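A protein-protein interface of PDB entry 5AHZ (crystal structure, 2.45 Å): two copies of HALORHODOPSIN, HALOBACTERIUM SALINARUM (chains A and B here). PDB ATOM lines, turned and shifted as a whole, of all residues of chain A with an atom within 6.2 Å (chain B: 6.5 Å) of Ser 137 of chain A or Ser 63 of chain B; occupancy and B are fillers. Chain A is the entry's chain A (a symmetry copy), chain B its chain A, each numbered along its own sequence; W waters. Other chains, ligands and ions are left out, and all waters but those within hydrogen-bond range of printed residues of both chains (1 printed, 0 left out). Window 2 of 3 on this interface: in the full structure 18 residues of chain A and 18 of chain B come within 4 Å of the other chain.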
ATOM      1  N   PRO A  73     -21.019 -14.023   9.383  1.00  0.00           N
ATOM      2  CA  PRO A  73     -20.104 -14.532  10.411  1.00  0.00           C
ATOM      3  C   PRO A  73     -20.598 -15.831  11.060  1.00  0.00           C
ATOM      4  O   PRO A  73     -21.795 -16.161  10.997  1.00  0.00           O
ATOM      5  CB  PRO A  73     -20.073 -13.396  11.432  1.00  0.00           C
ATOM      6  CG  PRO A  73     -21.457 -12.814  11.341  1.00  0.00           C
ATOM      7  CD  PRO A  73     -21.808 -12.875   9.869  1.00  0.00           C
ATOM      8  N   MET A 134     -23.088  -4.239   7.354  1.00  0.00           N
ATOM      9  CA  MET A 134     -21.718  -4.378   6.846  1.00  0.00           C
ATOM     10  C   MET A 134     -20.791  -5.189   7.774  1.00  0.00           C
ATOM     11  O   MET A 134     -19.793  -5.734   7.323  1.00  0.00           O
ATOM     12  CB  MET A 134     -21.087  -2.998   6.600  1.00  0.00           C
ATOM     13  CG  MET A 134     -21.807  -2.082   5.605  1.00  0.00           C
ATOM     14  SD  MET A 134     -21.760  -2.696   3.919  1.00  0.00           S
ATOM     15  CE  MET A 134     -23.284  -3.657   3.848  1.00  0.00           C
ATOM     16  N   THR A 135     -21.094  -5.251   9.068  1.00  0.00           N
ATOM     17  CA  THR A 135     -20.167  -5.895   9.995  1.00  0.00           C
ATOM     18  C   THR A 135     -20.051  -7.390   9.692  1.00  0.00           C
ATOM     19  O   THR A 135     -21.055  -8.106   9.605  1.00  0.00           O
ATOM     20  CB  THR A 135     -20.587  -5.692  11.466  1.00  0.00           C
ATOM     21  OG1 THR A 135     -20.362  -4.327  11.843  1.00  0.00           O
ATOM     22  CG2 THR A 135     -19.756  -6.578  12.372  1.00  0.00           C
ATOM     23  N   THR A 136     -18.824  -7.858   9.512  1.00  0.00           N
ATOM     24  CA  THR A 136     -18.606  -9.250   9.151  1.00  0.00           C
ATOM     25  C   THR A 136     -17.741 -10.017  10.161  1.00  0.00           C
ATOM     26  O   THR A 136     -17.659 -11.240  10.089  1.00  0.00           O
ATOM     27  CB  THR A 136     -17.918  -9.373   7.789  1.00  0.00           C
ATOM     28  OG1 THR A 136     -16.613  -8.808   7.889  1.00  0.00           O
ATOM     29  CG2 THR A 136     -18.684  -8.647   6.717  1.00  0.00           C
ATOM     30  N   SER A 137     -17.090  -9.309  11.082  1.00  0.00           N
ATOM     31  CA  SER A 137     -16.087  -9.945  11.952  1.00  0.00           C
ATOM     32  C   SER A 137     -16.693 -10.837  13.035  1.00  0.00           C
ATOM     33  O   SER A 137     -16.046 -11.782  13.465  1.00  0.00           O
ATOM     34  CB  SER A 137     -15.171  -8.886  12.600  1.00  0.00           C
ATOM     35  OG  SER A 137     -15.894  -7.934  13.382  1.00  0.00           O
ATOM     36  N   ALA A 138     -17.920 -10.545  13.471  1.00  0.00           N
ATOM     37  CA  ALA A 138     -18.587 -11.363  14.479  1.00  0.00           C
ATOM     38  C   ALA A 138     -20.073 -11.059  14.570  1.00  0.00           C
ATOM     39  O   ALA A 138     -20.498  -9.926  14.344  1.00  0.00           O
ATOM     40  CB  ALA A 138     -17.929 -11.170  15.856  1.00  0.00           C
ATOM     41  N   LEU A 139     -20.854 -12.079  14.929  1.00  0.00           N
ATOM     42  CA  LEU A 139     -22.303 -11.947  15.101  1.00  0.00           C
ATOM     43  C   LEU A 139     -22.683 -10.982  16.246  1.00  0.00           C
ATOM     44  O   LEU A 139     -23.666 -10.241  16.140  1.00  0.00           O
ATOM     45  CB  LEU A 139     -22.922 -13.328  15.340  1.00  0.00           C
ATOM     46  CG  LEU A 139     -24.420 -13.531  15.096  1.00  0.00           C
ATOM     47  CD1 LEU A 139     -24.836 -13.025  13.712  1.00  0.00           C
ATOM     48  CD2 LEU A 139     -24.766 -15.012  15.252  1.00  0.00           C
ATOM     49  N   PHE A 141     -21.292  -8.258  17.175  1.00  0.00           N
ATOM     50  CA  PHE A 141     -21.189  -6.879  16.745  1.00  0.00           C
ATOM     51  C   PHE A 141     -22.351  -6.473  15.869  1.00  0.00           C
ATOM     52  O   PHE A 141     -22.878  -5.387  16.049  1.00  0.00           O
ATOM     53  CB  PHE A 141     -19.854  -6.652  16.030  1.00  0.00           C
ATOM     54  CG  PHE A 141     -18.675  -6.680  16.959  1.00  0.00           C
ATOM     55  CD1 PHE A 141     -18.664  -5.894  18.106  1.00  0.00           C
ATOM     56  CD2 PHE A 141     -17.603  -7.516  16.719  1.00  0.00           C
ATOM     57  CE1 PHE A 141     -17.588  -5.926  18.994  1.00  0.00           C
ATOM     58  CE2 PHE A 141     -16.509  -7.555  17.607  1.00  0.00           C
ATOM     59  CZ  PHE A 141     -16.504  -6.757  18.738  1.00  0.00           C
ATOM     60  N   PHE A 145     -24.918  -3.367  17.041  1.00  0.00           N
ATOM     61  CA  PHE A 145     -25.233  -2.251  16.151  1.00  0.00           C
ATOM     62  C   PHE A 145     -26.734  -2.122  15.904  1.00  0.00           C
ATOM     63  O   PHE A 145     -27.278  -1.006  15.850  1.00  0.00           O
ATOM     64  CB  PHE A 145     -24.498  -2.407  14.820  1.00  0.00           C
ATOM     65  CG  PHE A 145     -23.134  -1.775  14.809  1.00  0.00           C
ATOM     66  CD1 PHE A 145     -22.955  -0.476  15.271  1.00  0.00           C
ATOM     67  CD2 PHE A 145     -22.029  -2.478  14.346  1.00  0.00           C
ATOM     68  CE1 PHE A 145     -21.703   0.125  15.257  1.00  0.00           C
ATOM     69  CE2 PHE A 145     -20.773  -1.893  14.336  1.00  0.00           C
ATOM     70  CZ  PHE A 145     -20.607  -0.581  14.796  1.00  0.00           C
ATOM     71  N   TYR B  58     -17.092   3.234  18.943  1.00  0.00           N
ATOM     72  CA  TYR B  58     -16.184   2.242  19.502  1.00  0.00           C
ATOM     73  C   TYR B  58     -16.579   0.830  19.080  1.00  0.00           C
ATOM     74  O   TYR B  58     -15.718  -0.046  18.993  1.00  0.00           O
ATOM     75  CB  TYR B  58     -16.106   2.366  21.034  1.00  0.00           C
ATOM     76  CG  TYR B  58     -15.163   3.477  21.494  1.00  0.00           C
ATOM     77  CD1 TYR B  58     -13.784   3.276  21.531  1.00  0.00           C
ATOM     78  CD2 TYR B  58     -15.653   4.726  21.894  1.00  0.00           C
ATOM     79  CE1 TYR B  58     -12.918   4.289  21.939  1.00  0.00           C
ATOM     80  CE2 TYR B  58     -14.797   5.738  22.310  1.00  0.00           C
ATOM     81  CZ  TYR B  58     -13.425   5.510  22.326  1.00  0.00           C
ATOM     82  OH  TYR B  58     -12.561   6.502  22.744  1.00  0.00           O
ATOM     83  N   LEU B  59     -17.864   0.599  18.801  1.00  0.00           N
ATOM     84  CA  LEU B  59     -18.250  -0.714  18.271  1.00  0.00           C
ATOM     85  C   LEU B  59     -17.678  -0.821  16.864  1.00  0.00           C
ATOM     86  O   LEU B  59     -17.204  -1.873  16.473  1.00  0.00           O
ATOM     87  CB  LEU B  59     -19.774  -0.925  18.267  1.00  0.00           C
ATOM     88  CG  LEU B  59     -20.498  -1.011  19.609  1.00  0.00           C
ATOM     89  CD1 LEU B  59     -22.016  -1.125  19.400  1.00  0.00           C
ATOM     90  CD2 LEU B  59     -19.958  -2.176  20.427  1.00  0.00           C
ATOM     91  N   GLY B  60     -17.701   0.286  16.123  1.00  0.00           N
ATOM     92  CA  GLY B  60     -17.013   0.370  14.833  1.00  0.00           C
ATOM     93  C   GLY B  60     -15.548  -0.063  14.824  1.00  0.00           C
ATOM     94  O   GLY B  60     -15.121  -0.880  13.988  1.00  0.00           O
ATOM     95  N   LEU B  61     -14.763   0.466  15.757  1.00  0.00           N
ATOM     96  CA  LEU B  61     -13.344   0.109  15.846  1.00  0.00           C
ATOM     97  C   LEU B  61     -13.107  -1.328  16.340  1.00  0.00           C
ATOM     98  O   LEU B  61     -12.253  -2.034  15.792  1.00  0.00           O
ATOM     99  CB  LEU B  61     -12.614   1.104  16.756  1.00  0.00           C
ATOM    100  CG  LEU B  61     -12.753   2.585  16.362  1.00  0.00           C
ATOM    101  CD1 LEU B  61     -12.559   3.460  17.571  1.00  0.00           C
ATOM    102  CD2 LEU B  61     -11.751   2.964  15.269  1.00  0.00           C
ATOM    103  N   LEU B  62     -13.848  -1.761  17.365  1.00  0.00           N
ATOM    104  CA  LEU B  62     -13.701  -3.132  17.904  1.00  0.00           C
ATOM    105  C   LEU B  62     -13.943  -4.216  16.867  1.00  0.00           C
ATOM    106  O   LEU B  62     -13.250  -5.222  16.852  1.00  0.00           O
ATOM    107  CB  LEU B  62     -14.659  -3.377  19.068  1.00  0.00           C
ATOM    108  CG  LEU B  62     -14.272  -2.869  20.452  1.00  0.00           C
ATOM    109  CD1 LEU B  62     -15.462  -3.001  21.373  1.00  0.00           C
ATOM    110  CD2 LEU B  62     -13.087  -3.672  20.981  1.00  0.00           C
ATOM    111  N   SER B  63     -14.929  -4.000  16.001  1.00  0.00           N
ATOM    112  CA  SER B  63     -15.323  -4.983  14.997  1.00  0.00           C
ATOM    113  C   SER B  63     -14.428  -4.994  13.743  1.00  0.00           C
ATOM    114  O   SER B  63     -14.576  -5.855  12.872  1.00  0.00           O
ATOM    115  CB  SER B  63     -16.779  -4.730  14.582  1.00  0.00           C
ATOM    116  OG  SER B  63     -16.932  -3.458  13.960  1.00  0.00           O
ATOM    117  N   GLY B  64     -13.512  -4.032  13.656  1.00  0.00           N
ATOM    118  CA  GLY B  64     -12.627  -3.895  12.511  1.00  0.00           C
ATOM    119  C   GLY B  64     -13.246  -3.119  11.362  1.00  0.00           C
ATOM    120  O   GLY B  64     -12.578  -2.805  10.378  1.00  0.00           O
ATOM    121  N   LEU B  65     -14.529  -2.806  11.484  1.00  0.00           N
ATOM    122  CA  LEU B  65     -15.245  -2.166  10.396  1.00  0.00           C
ATOM    123  C   LEU B  65     -14.603  -0.848  10.015  1.00  0.00           C
ATOM    124  O   LEU B  65     -14.521  -0.504   8.844  1.00  0.00           O
ATOM    125  CB  LEU B  65     -16.698  -1.940  10.782  1.00  0.00           C
ATOM    126  CG  LEU B  65     -17.609  -1.453   9.657  1.00  0.00           C
ATOM    127  CD1 LEU B  65     -17.988  -2.622   8.744  1.00  0.00           C
ATOM    128  CD2 LEU B  65     -18.841  -0.778  10.233  1.00  0.00           C
ATOM    129  N   THR B  66     -14.140  -0.101  11.007  1.00  0.00           N
ATOM    130  CA  THR B  66     -13.585   1.223  10.731  1.00  0.00           C
ATOM    131  C   THR B  66     -12.077   1.347  11.083  1.00  0.00           C
ATOM    132  O   THR B  66     -11.584   2.435  11.409  1.00  0.00           O
ATOM    133  CB  THR B  66     -14.408   2.303  11.472  1.00  0.00           C
ATOM    134  OG1 THR B  66     -14.363   2.064  12.882  1.00  0.00           O
ATOM    135  CG2 THR B  66     -15.866   2.298  11.016  1.00  0.00           C
ATOM    136  N   VAL B  67     -11.349   0.229  11.002  1.00  0.00           N
ATOM    137  CA  VAL B  67      -9.894   0.240  11.197  1.00  0.00           C
ATOM    138  C   VAL B  67      -9.234  -0.233   9.900  1.00  0.00           C
ATOM    139  O   VAL B  67      -9.734  -1.148   9.255  1.00  0.00           O
ATOM    140  CB  VAL B  67      -9.430  -0.670  12.381  1.00  0.00           C
ATOM    141  CG1 VAL B  67      -7.916  -0.591  12.573  1.00  0.00           C
ATOM    142  CG2 VAL B  67     -10.132  -0.298  13.684  1.00  0.00           C
HETATM  143  O   HOH W   1     -16.120  -6.358  10.395  1.00  0.00           O
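Water W1 lies within hydrogen-bond range of O of Ser 63 of chain B (3.0 Å), N of Ser 137 of chain A (3.2 Å) and N of Thr 136 of chain A (3.2 Å).
The backbone carbonyl oxygen (O) of Ser 63 of chain B lies within hydrogen-bond range of the side-chain hydroxyl (OG) of Ser 137 of chain A (2.5 Å).
Of chain B, only Ser 63 comes within 4 Å of Ser 137 of chain A.
Of the printed residues of chain B, Phe 141 of chain A touches Leu 62 and Ser 63.
Of the printed residues of chain A, Leu 59 of chain B touches Phe 145.
Of the printed residues of chain A, Gly 60 of chain B touches Phe 145.
Ser 63 of chain B touches two residues of chain A.
Among the printed residues, merely in contact across the chains: Phe 145 of chain A with Gly 60 of chain B (3.3 Å), Phe 145 of chain A with Leu 59 of chain B (3.6 Å), Phe 141 of chain A with Ser 63 of chain B (3.6 Å), Met 134 of chain A with Leu 65 of chain B (3.8 Å) and Phe 141 of chain A with Leu 62 of chain B (3.9 Å).
No position is printed for both chains.
Of the 6 pairs that touch across the chains among the printed residues, none has its exchanged pair printed and touching as well.
OG of Ser 63 of chain B is in hydrogen-bond range of O of Gly 60 of chain B (3.2 Å).
The side-chain hydroxyl (OG) of Ser 63 of chain B is in hydrogen-bond range of the backbone carbonyl oxygen (O) of Leu 59 of chain B (3.0 Å).
The backbone NH of Leu 65 of chain B lies within hydrogen-bond range of the backbone carbonyl oxygen of Gly 60 of chain B.
The backbone carbonyl oxygen (O) of Gly 60 of chain B lies within hydrogen-bond range of the backbone NH (N) of Thr 66 of chain B, 3.2 Å away.
Hydrophobic or aromatic side chains of chain B that line the printed part of chain A: Leu 59, Leu 62 and Leu 65.
Printed residues of chain A that touch a printed residue of chain B: Met 134, Ser 137, Phe 141 and Phe 145.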
